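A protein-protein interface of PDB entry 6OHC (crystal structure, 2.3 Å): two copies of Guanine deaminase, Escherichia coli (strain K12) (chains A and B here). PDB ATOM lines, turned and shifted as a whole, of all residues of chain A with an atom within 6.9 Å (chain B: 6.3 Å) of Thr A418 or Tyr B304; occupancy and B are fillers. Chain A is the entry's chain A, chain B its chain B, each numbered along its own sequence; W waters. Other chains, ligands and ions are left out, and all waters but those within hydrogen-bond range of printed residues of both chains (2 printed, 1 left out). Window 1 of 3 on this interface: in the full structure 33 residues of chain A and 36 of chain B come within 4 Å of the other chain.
Printed residues of chain B that touch a printed residue of chain A: Leu B303, Tyr B304, Leu B305, Gly B306, Gly B331, Thr B332 and Glu B342.
Of the 19 printed residues of chain A, 8 touch a printed residue of chain B.
Water W2 lies within hydrogen-bond range of OH of Tyr B304, ND2 of Asn A341, NZ of Lys A345 and OG1 of Thr B332.
Water W1 bridges the guanidinium group (NH1) of Arg A402 and the backbone carbonyl oxygen (O) of Ala B330.
The side-chain amino group (NZ) of Lys A345 lies close to the side-chain amide nitrogen (ND2) of Asn A341, at 3.5 Å.
The side-chain amino group (NZ) of Lys A345 lies within salt-bridge range of the side-chain carboxylate (OE2) of Glu A342, 2.7 Å away.
OH of Tyr B304 sits at hydrogen-bond distance from OG1 of Thr B332, 3.0 Å away.
The side-chain hydroxyl (OH) of Tyr A344 sits at hydrogen-bond distance from the side-chain amide nitrogen (NE2) of Gln A348, at 3.1 Å.
The backbone carbonyl oxygen of Phe A414 is in hydrogen-bond range of the side-chain hydroxyl of Thr A418, at 2.8 Å.
Printed residues of chain B within 4 Å of Glu A342: Glu B342.
Printed residues of chain B within 4 Å of Gln A348: Leu B303, Tyr B304, Leu B305 and Gly B306.
Met A416 touches none of the printed residues of chain B.
Met A417 touches none of the printed residues of chain B.
Thr A418 touches two residues of chain B.
Of the printed residues of chain A, Tyr B304 touches Asn A341 (2.6 Å), Tyr A344 (3.6 Å), Gln A348 (3.3 Å) and Thr A418 (3.4 Å).
Printed residues of chain A within 4 Å of Gly B331: Arg A402 (3.6 Å).
The nearest printed residue of chain B that does not touch Thr A418 is Gly B331 (7.3 Å).
The nearest residue of chain A that does not touch Tyr B304 is Lys A345 (4.2 Å).
Glu A342 touches Glu B342.
CE1 of Tyr A344 touches O of Tyr B304, 3.6 Å away.
Lys A345 touches Leu B303 (CD to CB, 3.7 Å).
Leu B303 touches Gln A348 (O to CB, 3.5 Å).
Gln A348 touches Leu B305 (OE1 to C, 3.9 Å).
Gly B306 touches Gln A348 (CA to O, 3.8 Å).
Arg A402 touches Gly B331 (NH2 to O, 3.6 Å).
CG2 of Thr B332 touches NH1 of Arg A402, at 3.9 Å.
Thr A418 touches Thr B332 (O to CB, 3.8 Å).
CG of Leu A419 touches O of Thr B332 (3.7 Å).
The backbone carbonyl oxygen (O) of Thr A418 is in hydrogen-bond range of the side-chain hydroxyl (OH) of Tyr B304, 3.4 Å away.
The side-chain amide oxygen (OE1) of Gln A348 lies close to the backbone carbonyl oxygen (O) of Tyr B304 (3.4 Å).
The side-chain carboxylate of Glu B342 lies within salt-bridge range of the side-chain amino group of Lys A345 (2.8 Å).
OH of Tyr B304 sits at hydrogen-bond distance from OD1 of Asn A341.
Glu A342 touches its own counterpart, Glu B342.
Position printed for both chains: 342.
Of the 14 pairs that touch across the chains among the printed residues, 1 has its exchanged pair printed and touching as well.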
ATOM      1  N   LEU A 337     -14.957 -16.223  -9.746  1.00  0.00           N
ATOM      2  CA  LEU A 337     -14.007 -15.385 -10.554  1.00  0.00           C
ATOM      3  C   LEU A 337     -13.198 -16.299 -11.493  1.00  0.00           C
ATOM      4  O   LEU A 337     -13.143 -15.981 -12.669  1.00  0.00           O
ATOM      5  CB  LEU A 337     -13.075 -14.622  -9.636  1.00  0.00           C
ATOM      6  CG  LEU A 337     -13.718 -13.740  -8.604  1.00  0.00           C
ATOM      7  CD1 LEU A 337     -12.611 -13.255  -7.635  1.00  0.00           C
ATOM      8  CD2 LEU A 337     -14.420 -12.590  -9.269  1.00  0.00           C
ATOM      9  N   GLN A 338     -12.660 -17.431 -10.974  1.00  0.00           N
ATOM     10  CA  GLN A 338     -11.947 -18.427 -11.802  1.00  0.00           C
ATOM     11  C   GLN A 338     -12.893 -19.007 -12.847  1.00  0.00           C
ATOM     12  O   GLN A 338     -12.452 -19.223 -13.955  1.00  0.00           O
ATOM     13  CB  GLN A 338     -11.330 -19.507 -10.927  1.00  0.00           C
ATOM     14  CG  GLN A 338     -10.235 -18.934 -10.036  1.00  0.00           C
ATOM     15  CD  GLN A 338      -9.455 -20.021  -9.348  1.00  0.00           C
ATOM     16  OE1 GLN A 338     -10.046 -21.015  -8.904  1.00  0.00           O
ATOM     17  NE2 GLN A 338      -8.151 -19.874  -9.287  1.00  0.00           N
ATOM     18  N   LEU A 340     -15.414 -17.518 -14.329  1.00  0.00           N
ATOM     19  CA  LEU A 340     -15.517 -16.466 -15.375  1.00  0.00           C
ATOM     20  C   LEU A 340     -14.247 -16.452 -16.184  1.00  0.00           C
ATOM     21  O   LEU A 340     -14.358 -16.294 -17.374  1.00  0.00           O
ATOM     22  CB  LEU A 340     -15.762 -15.109 -14.714  1.00  0.00           C
ATOM     23  CG  LEU A 340     -17.099 -15.034 -13.992  1.00  0.00           C
ATOM     24  CD1 LEU A 340     -17.135 -13.721 -13.177  1.00  0.00           C
ATOM     25  CD2 LEU A 340     -18.276 -15.225 -15.008  1.00  0.00           C
ATOM     26  N   ASN A 341     -13.100 -16.656 -15.544  1.00  0.00           N
ATOM     27  CA  ASN A 341     -11.792 -16.718 -16.258  1.00  0.00           C
ATOM     28  C   ASN A 341     -11.877 -17.853 -17.289  1.00  0.00           C
ATOM     29  O   ASN A 341     -11.379 -17.644 -18.421  1.00  0.00           O
ATOM     30  CB  ASN A 341     -10.613 -16.903 -15.314  1.00  0.00           C
ATOM     31  CG  ASN A 341      -9.264 -16.729 -15.996  1.00  0.00           C
ATOM     32  OD1 ASN A 341      -9.036 -15.786 -16.763  1.00  0.00           O
ATOM     33  ND2 ASN A 341      -8.348 -17.616 -15.709  1.00  0.00           N
ATOM     34  N   GLU A 342     -12.528 -18.989 -16.952  1.00  0.00           N
ATOM     35  CA  GLU A 342     -12.530 -20.161 -17.846  1.00  0.00           C
ATOM     36  C   GLU A 342     -13.527 -19.882 -18.972  1.00  0.00           C
ATOM     37  O   GLU A 342     -13.280 -20.320 -20.123  1.00  0.00           O
ATOM     38  CB  GLU A 342     -12.888 -21.447 -17.082  1.00  0.00           C
ATOM     39  CG  GLU A 342     -11.865 -21.801 -16.026  1.00  0.00           C
ATOM     40  CD  GLU A 342     -10.431 -21.927 -16.531  1.00  0.00           C
ATOM     41  OE1 GLU A 342     -10.233 -22.659 -17.521  1.00  0.00           O
ATOM     42  OE2 GLU A 342      -9.529 -21.316 -15.939  1.00  0.00           O
ATOM     43  N   TYR A 344     -14.101 -16.936 -20.235  1.00  0.00           N
ATOM     44  CA  TYR A 344     -13.304 -16.063 -21.134  1.00  0.00           C
ATOM     45  C   TYR A 344     -12.515 -16.924 -22.113  1.00  0.00           C
ATOM     46  O   TYR A 344     -12.532 -16.628 -23.290  1.00  0.00           O
ATOM     47  CB  TYR A 344     -12.421 -15.145 -20.317  1.00  0.00           C
ATOM     48  CG  TYR A 344     -11.719 -14.096 -21.130  1.00  0.00           C
ATOM     49  CD1 TYR A 344     -10.447 -14.306 -21.638  1.00  0.00           C
ATOM     50  CD2 TYR A 344     -12.319 -12.870 -21.376  1.00  0.00           C
ATOM     51  CE1 TYR A 344      -9.797 -13.328 -22.378  1.00  0.00           C
ATOM     52  CE2 TYR A 344     -11.690 -11.897 -22.139  1.00  0.00           C
ATOM     53  CZ  TYR A 344     -10.427 -12.125 -22.638  1.00  0.00           C
ATOM     54  OH  TYR A 344      -9.813 -11.137 -23.347  1.00  0.00           O
ATOM     55  N   LYS A 345     -11.909 -18.010 -21.629  1.00  0.00           N
ATOM     56  CA  LYS A 345     -11.012 -18.891 -22.402  1.00  0.00           C
ATOM     57  C   LYS A 345     -11.843 -19.706 -23.382  1.00  0.00           C
ATOM     58  O   LYS A 345     -11.495 -19.734 -24.563  1.00  0.00           O
ATOM     59  CB  LYS A 345     -10.114 -19.693 -21.458  1.00  0.00           C
ATOM     60  CG  LYS A 345      -8.993 -18.863 -20.865  1.00  0.00           C
ATOM     61  CD  LYS A 345      -8.035 -19.601 -19.971  1.00  0.00           C
ATOM     62  CE  LYS A 345      -8.680 -19.967 -18.661  1.00  0.00           C
ATOM     63  NZ  LYS A 345      -7.686 -20.414 -17.656  1.00  0.00           N
ATOM     64  N   GLN A 348     -12.973 -17.279 -26.064  1.00  0.00           N
ATOM     65  CA  GLN A 348     -11.923 -16.758 -26.979  1.00  0.00           C
ATOM     66  C   GLN A 348     -11.648 -17.800 -28.070  1.00  0.00           C
ATOM     67  O   GLN A 348     -11.314 -17.407 -29.192  1.00  0.00           O
ATOM     68  CB  GLN A 348     -10.611 -16.476 -26.251  1.00  0.00           C
ATOM     69  CG  GLN A 348     -10.649 -15.231 -25.376  1.00  0.00           C
ATOM     70  CD  GLN A 348     -10.394 -13.973 -26.166  1.00  0.00           C
ATOM     71  OE1 GLN A 348      -9.770 -14.002 -27.223  1.00  0.00           O
ATOM     72  NE2 GLN A 348     -10.950 -12.884 -25.684  1.00  0.00           N
ATOM     73  N   GLN A 399      -1.783  -9.769  -8.867  1.00  0.00           N
ATOM     74  CA  GLN A 399      -3.136  -9.190  -8.863  1.00  0.00           C
ATOM     75  C   GLN A 399      -3.085  -7.749  -8.333  1.00  0.00           C
ATOM     76  O   GLN A 399      -3.794  -6.911  -8.892  1.00  0.00           O
ATOM     77  CB  GLN A 399      -4.113 -10.052  -8.055  1.00  0.00           C
ATOM     78  CG  GLN A 399      -5.532  -9.691  -8.425  1.00  0.00           C
ATOM     79  CD  GLN A 399      -6.620 -10.391  -7.648  1.00  0.00           C
ATOM     80  OE1 GLN A 399      -7.733 -10.477  -8.143  1.00  0.00           O
ATOM     81  NE2 GLN A 399      -6.353 -10.845  -6.446  1.00  0.00           N
ATOM     82  N   ARG A 402      -1.533  -5.528 -10.978  1.00  0.00           N
ATOM     83  CA  ARG A 402      -2.356  -5.241 -12.172  1.00  0.00           C
ATOM     84  C   ARG A 402      -3.490  -4.300 -11.765  1.00  0.00           C
ATOM     85  O   ARG A 402      -3.916  -3.473 -12.589  1.00  0.00           O
ATOM     86  CB  ARG A 402      -2.855  -6.522 -12.836  1.00  0.00           C
ATOM     87  CG  ARG A 402      -1.742  -7.324 -13.497  1.00  0.00           C
ATOM     88  CD  ARG A 402      -2.254  -8.443 -14.400  1.00  0.00           C
ATOM     89  NE  ARG A 402      -1.111  -8.909 -15.148  1.00  0.00           N
ATOM     90  CZ  ARG A 402      -1.127  -9.752 -16.161  1.00  0.00           C
ATOM     91  NH1 ARG A 402      -2.256 -10.255 -16.611  1.00  0.00           N
ATOM     92  NH2 ARG A 402       0.008 -10.054 -16.780  1.00  0.00           N
ATOM     93  N   ASP A 411     -11.308  -2.445 -16.378  1.00  0.00           N
ATOM     94  CA  ASP A 411      -9.943  -2.977 -16.140  1.00  0.00           C
ATOM     95  C   ASP A 411      -9.884  -3.595 -14.744  1.00  0.00           C
ATOM     96  O   ASP A 411      -9.322  -4.675 -14.625  1.00  0.00           O
ATOM     97  CB  ASP A 411      -8.856  -1.927 -16.343  1.00  0.00           C
ATOM     98  CG  ASP A 411      -8.418  -1.738 -17.786  1.00  0.00           C
ATOM     99  OD1 ASP A 411      -9.024  -2.344 -18.666  1.00  0.00           O
ATOM    100  OD2 ASP A 411      -7.395  -1.004 -18.008  1.00  0.00           O
ATOM    101  N   LEU A 413     -12.491  -4.803 -12.994  1.00  0.00           N
ATOM    102  CA  LEU A 413     -13.311  -6.050 -13.084  1.00  0.00           C
ATOM    103  C   LEU A 413     -12.477  -7.154 -13.765  1.00  0.00           C
ATOM    104  O   LEU A 413     -12.564  -8.310 -13.390  1.00  0.00           O
ATOM    105  CB  LEU A 413     -14.595  -5.775 -13.885  1.00  0.00           C
ATOM    106  CG  LEU A 413     -15.726  -5.213 -13.055  1.00  0.00           C
ATOM    107  CD1 LEU A 413     -16.978  -5.037 -13.875  1.00  0.00           C
ATOM    108  CD2 LEU A 413     -16.001  -6.156 -11.916  1.00  0.00           C
ATOM    109  N   PHE A 414     -11.678  -6.773 -14.750  1.00  0.00           N
ATOM    110  CA  PHE A 414     -10.894  -7.723 -15.571  1.00  0.00           C
ATOM    111  C   PHE A 414      -9.808  -8.331 -14.688  1.00  0.00           C
ATOM    112  O   PHE A 414      -9.567  -9.559 -14.779  1.00  0.00           O
ATOM    113  CB  PHE A 414     -10.258  -7.035 -16.782  1.00  0.00           C
ATOM    114  CG  PHE A 414      -9.563  -7.978 -17.724  1.00  0.00           C
ATOM    115  CD1 PHE A 414     -10.312  -8.689 -18.638  1.00  0.00           C
ATOM    116  CD2 PHE A 414      -8.175  -8.043 -17.812  1.00  0.00           C
ATOM    117  CE1 PHE A 414      -9.700  -9.472 -19.608  1.00  0.00           C
ATOM    118  CE2 PHE A 414      -7.569  -8.879 -18.732  1.00  0.00           C
ATOM    119  CZ  PHE A 414      -8.333  -9.576 -19.636  1.00  0.00           C
ATOM    120  N   VAL A 415      -9.144  -7.506 -13.871  1.00  0.00           N
ATOM    121  CA  VAL A 415      -8.081  -7.998 -12.958  1.00  0.00           C
ATOM    122  C   VAL A 415      -8.711  -8.921 -11.910  1.00  0.00           C
ATOM    123  O   VAL A 415      -8.092  -9.939 -11.581  1.00  0.00           O
ATOM    124  CB  VAL A 415      -7.264  -6.862 -12.356  1.00  0.00           C
ATOM    125  CG1 VAL A 415      -6.324  -7.360 -11.255  1.00  0.00           C
ATOM    126  CG2 VAL A 415      -6.456  -6.209 -13.467  1.00  0.00           C
ATOM    127  N   MET A 416      -9.921  -8.636 -11.441  1.00  0.00           N
ATOM    128  CA  MET A 416     -10.602  -9.492 -10.452  1.00  0.00           C
ATOM    129  C   MET A 416     -10.946 -10.839 -11.096  1.00  0.00           C
ATOM    130  O   MET A 416     -10.781 -11.853 -10.431  1.00  0.00           O
ATOM    131  CB  MET A 416     -11.866  -8.798  -9.964  1.00  0.00           C
ATOM    132  CG  MET A 416     -11.614  -7.558  -9.133  1.00  0.00           C
ATOM    133  SD  MET A 416     -10.452  -7.750  -7.742  1.00  0.00           S
ATOM    134  CE  MET A 416     -11.313  -9.026  -6.835  1.00  0.00           C
ATOM    135  N   MET A 417     -11.417 -10.838 -12.346  1.00  0.00           N
ATOM    136  CA  MET A 417     -11.789 -12.045 -13.136  1.00  0.00           C
ATOM    137  C   MET A 417     -10.547 -12.883 -13.477  1.00  0.00           C
ATOM    138  O   MET A 417     -10.604 -14.121 -13.282  1.00  0.00           O
ATOM    139  CB  MET A 417     -12.504 -11.653 -14.421  1.00  0.00           C
ATOM    140  CG  MET A 417     -12.673 -12.805 -15.427  1.00  0.00           C
ATOM    141  SD  MET A 417     -13.718 -12.356 -16.875  1.00  0.00           S
ATOM    142  CE  MET A 417     -12.499 -11.707 -18.023  1.00  0.00           C
ATOM    143  N   THR A 418      -9.454 -12.278 -13.928  1.00  0.00           N
ATOM    144  CA  THR A 418      -8.352 -13.045 -14.571  1.00  0.00           C
ATOM    145  C   THR A 418      -7.328 -13.538 -13.554  1.00  0.00           C
ATOM    146  O   THR A 418      -6.619 -14.507 -13.903  1.00  0.00           O
ATOM    147  CB  THR A 418      -7.677 -12.302 -15.745  1.00  0.00           C
ATOM    148  OG1 THR A 418      -7.206 -10.988 -15.392  1.00  0.00           O
ATOM    149  CG2 THR A 418      -8.650 -12.293 -16.921  1.00  0.00           C
ATOM    150  N   LEU A 419      -7.167 -12.858 -12.411  1.00  0.00           N
ATOM    151  CA  LEU A 419      -6.179 -13.229 -11.371  1.00  0.00           C
ATOM    152  C   LEU A 419      -6.832 -13.429 -10.000  1.00  0.00           C
ATOM    153  O   LEU A 419      -6.125 -13.569  -9.032  1.00  0.00           O
ATOM    154  CB  LEU A 419      -5.132 -12.130 -11.276  1.00  0.00           C
ATOM    155  CG  LEU A 419      -4.072 -12.122 -12.377  1.00  0.00           C
ATOM    156  CD1 LEU A 419      -4.574 -11.381 -13.606  1.00  0.00           C
ATOM    157  CD2 LEU A 419      -2.818 -11.466 -11.824  1.00  0.00           C
ATOM    158  N   GLY A 420      -8.153 -13.446  -9.905  1.00  0.00           N
ATOM    159  CA  GLY A 420      -8.866 -13.701  -8.641  1.00  0.00           C
ATOM    160  C   GLY A 420      -8.903 -15.179  -8.293  1.00  0.00           C
ATOM    161  O   GLY A 420      -8.878 -16.007  -9.224  1.00  0.00           O
ATOM    162  N   PRO B 299       0.318 -22.737 -22.828  1.00  0.00           N
ATOM    163  CA  PRO B 299      -1.112 -22.964 -22.935  1.00  0.00           C
ATOM    164  C   PRO B 299      -1.954 -21.770 -22.473  1.00  0.00           C
ATOM    165  O   PRO B 299      -2.929 -21.472 -23.115  1.00  0.00           O
ATOM    166  CB  PRO B 299      -1.368 -24.199 -22.017  1.00  0.00           C
ATOM    167  CG  PRO B 299      -0.154 -24.263 -21.104  1.00  0.00           C
ATOM    168  CD  PRO B 299       0.979 -23.708 -21.956  1.00  0.00           C
ATOM    169  N   THR B 300      -1.602 -21.154 -21.350  1.00  0.00           N
ATOM    170  CA  THR B 300      -2.394 -20.067 -20.712  1.00  0.00           C
ATOM    171  C   THR B 300      -2.592 -18.905 -21.688  1.00  0.00           C
ATOM    172  O   THR B 300      -3.742 -18.509 -21.862  1.00  0.00           O
ATOM    173  CB  THR B 300      -1.727 -19.593 -19.409  1.00  0.00           C
ATOM    174  OG1 THR B 300      -1.414 -20.782 -18.689  1.00  0.00           O
ATOM    175  CG2 THR B 300      -2.581 -18.645 -18.573  1.00  0.00           C
ATOM    176  N   SER B 301      -1.524 -18.391 -22.305  1.00  0.00           N
ATOM    177  CA  SER B 301      -1.638 -17.299 -23.289  1.00  0.00           C
ATOM    178  C   SER B 301      -2.340 -17.848 -24.517  1.00  0.00           C
ATOM    179  O   SER B 301      -3.157 -17.119 -25.096  1.00  0.00           O
ATOM    180  CB  SER B 301      -0.282 -16.615 -23.651  1.00  0.00           C
ATOM    181  OG  SER B 301       0.658 -17.607 -23.990  1.00  0.00           O
ATOM    182  N   ASN B 302      -2.048 -19.081 -24.924  1.00  0.00           N
ATOM    183  CA  ASN B 302      -2.706 -19.641 -26.144  1.00  0.00           C
ATOM    184  C   ASN B 302      -4.239 -19.595 -25.945  1.00  0.00           C
ATOM    185  O   ASN B 302      -4.952 -19.368 -26.943  1.00  0.00           O
ATOM    186  CB  ASN B 302      -2.185 -21.042 -26.522  1.00  0.00           C
ATOM    187  CG  ASN B 302      -0.720 -21.062 -26.893  1.00  0.00           C
ATOM    188  OD1 ASN B 302      -0.092 -19.983 -27.100  1.00  0.00           O
ATOM    189  ND2 ASN B 302      -0.170 -22.266 -26.928  1.00  0.00           N
ATOM    190  N   LEU B 303      -4.733 -19.772 -24.714  1.00  0.00           N
ATOM    191  CA  LEU B 303      -6.191 -19.781 -24.464  1.00  0.00           C
ATOM    192  C   LEU B 303      -6.681 -18.334 -24.349  1.00  0.00           C
ATOM    193  O   LEU B 303      -7.775 -18.016 -24.851  1.00  0.00           O
ATOM    194  CB  LEU B 303      -6.530 -20.570 -23.200  1.00  0.00           C
ATOM    195  CG  LEU B 303      -6.449 -22.088 -23.265  1.00  0.00           C
ATOM    196  CD1 LEU B 303      -6.809 -22.695 -21.934  1.00  0.00           C
ATOM    197  CD2 LEU B 303      -7.349 -22.647 -24.355  1.00  0.00           C
ATOM    198  N   TYR B 304      -5.931 -17.482 -23.680  1.00  0.00           N
ATOM    199  CA  TYR B 304      -6.389 -16.096 -23.399  1.00  0.00           C
ATOM    200  C   TYR B 304      -6.498 -15.297 -24.716  1.00  0.00           C
ATOM    201  O   TYR B 304      -7.402 -14.426 -24.828  1.00  0.00           O
ATOM    202  CB  TYR B 304      -5.459 -15.386 -22.417  1.00  0.00           C
ATOM    203  CG  TYR B 304      -5.843 -15.562 -20.973  1.00  0.00           C
ATOM    204  CD1 TYR B 304      -7.066 -15.178 -20.440  1.00  0.00           C
ATOM    205  CD2 TYR B 304      -4.902 -16.093 -20.116  1.00  0.00           C
ATOM    206  CE1 TYR B 304      -7.318 -15.296 -19.081  1.00  0.00           C
ATOM    207  CE2 TYR B 304      -5.154 -16.249 -18.766  1.00  0.00           C
ATOM    208  CZ  TYR B 304      -6.356 -15.840 -18.240  1.00  0.00           C
ATOM    209  OH  TYR B 304      -6.424 -16.047 -16.886  1.00  0.00           O
ATOM    210  N   LEU B 305      -5.622 -15.574 -25.677  1.00  0.00           N
ATOM    211  CA  LEU B 305      -5.592 -14.843 -26.971  1.00  0.00           C
ATOM    212  C   LEU B 305      -6.327 -15.664 -28.036  1.00  0.00           C
ATOM    213  O   LEU B 305      -6.443 -15.186 -29.154  1.00  0.00           O
ATOM    214  CB  LEU B 305      -4.145 -14.565 -27.379  1.00  0.00           C
ATOM    215  CG  LEU B 305      -3.315 -13.791 -26.347  1.00  0.00           C
ATOM    216  CD1 LEU B 305      -1.984 -13.334 -26.917  1.00  0.00           C
ATOM    217  CD2 LEU B 305      -4.082 -12.606 -25.823  1.00  0.00           C
ATOM    218  N   GLY B 306      -6.830 -16.843 -27.682  1.00  0.00           N
ATOM    219  CA  GLY B 306      -7.545 -17.716 -28.621  1.00  0.00           C
ATOM    220  C   GLY B 306      -6.648 -18.111 -29.776  1.00  0.00           C
ATOM    221  O   GLY B 306      -7.193 -18.297 -30.875  1.00  0.00           O
ATOM    222  N   SER B 307      -5.345 -18.294 -29.529  1.00  0.00           N
ATOM    223  CA  SER B 307      -4.349 -18.735 -30.533  1.00  0.00           C
ATOM    224  C   SER B 307      -4.607 -20.186 -30.970  1.00  0.00           C
ATOM    225  O   SER B 307      -4.311 -20.502 -32.142  1.00  0.00           O
ATOM    226  CB  SER B 307      -2.956 -18.579 -30.008  1.00  0.00           C
ATOM    227  OG  SER B 307      -2.694 -17.221 -29.691  1.00  0.00           O
ATOM    228  N   ALA B 330       1.007 -12.054 -21.254  1.00  0.00           N
ATOM    229  CA  ALA B 330      -0.160 -12.575 -21.959  1.00  0.00           C
ATOM    230  C   ALA B 330      -0.814 -13.631 -21.027  1.00  0.00           C
ATOM    231  O   ALA B 330      -2.071 -13.651 -20.936  1.00  0.00           O
ATOM    232  CB  ALA B 330       0.354 -13.078 -23.273  1.00  0.00           C
ATOM    233  N   GLY B 331       0.018 -14.410 -20.332  1.00  0.00           N
ATOM    234  CA  GLY B 331      -0.394 -15.324 -19.270  1.00  0.00           C
ATOM    235  C   GLY B 331      -0.596 -14.558 -17.972  1.00  0.00           C
ATOM    236  O   GLY B 331       0.032 -13.509 -17.811  1.00  0.00           O
ATOM    237  N   THR B 332      -1.401 -15.110 -17.077  1.00  0.00           N
ATOM    238  CA  THR B 332      -1.850 -14.437 -15.860  1.00  0.00           C
ATOM    239  C   THR B 332      -1.208 -15.019 -14.595  1.00  0.00           C
ATOM    240  O   THR B 332      -1.587 -14.561 -13.484  1.00  0.00           O
ATOM    241  CB  THR B 332      -3.376 -14.557 -15.795  1.00  0.00           C
ATOM    242  OG1 THR B 332      -3.606 -15.960 -15.917  1.00  0.00           O
ATOM    243  CG2 THR B 332      -3.996 -13.726 -16.885  1.00  0.00           C
ATOM    244  N   GLU B 342      -3.444 -25.775 -17.178  1.00  0.00           N
ATOM    245  CA  GLU B 342      -3.991 -25.219 -18.449  1.00  0.00           C
ATOM    246  C   GLU B 342      -3.596 -26.159 -19.588  1.00  0.00           C
ATOM    247  O   GLU B 342      -4.390 -26.345 -20.529  1.00  0.00           O
ATOM    248  CB  GLU B 342      -3.479 -23.805 -18.716  1.00  0.00           C
ATOM    249  CG  GLU B 342      -3.870 -22.810 -17.640  1.00  0.00           C
ATOM    250  CD  GLU B 342      -5.370 -22.659 -17.516  1.00  0.00           C
ATOM    251  OE1 GLU B 342      -6.003 -22.445 -18.546  1.00  0.00           O
ATOM    252  OE2 GLU B 342      -5.875 -22.751 -16.397  1.00  0.00           O
HETATM  253  O   HOH W   1      -2.811 -11.242 -19.292  1.00  0.00           O
HETATM  254  O   HOH W   2      -5.634 -18.635 -15.889  1.00  0.00           O
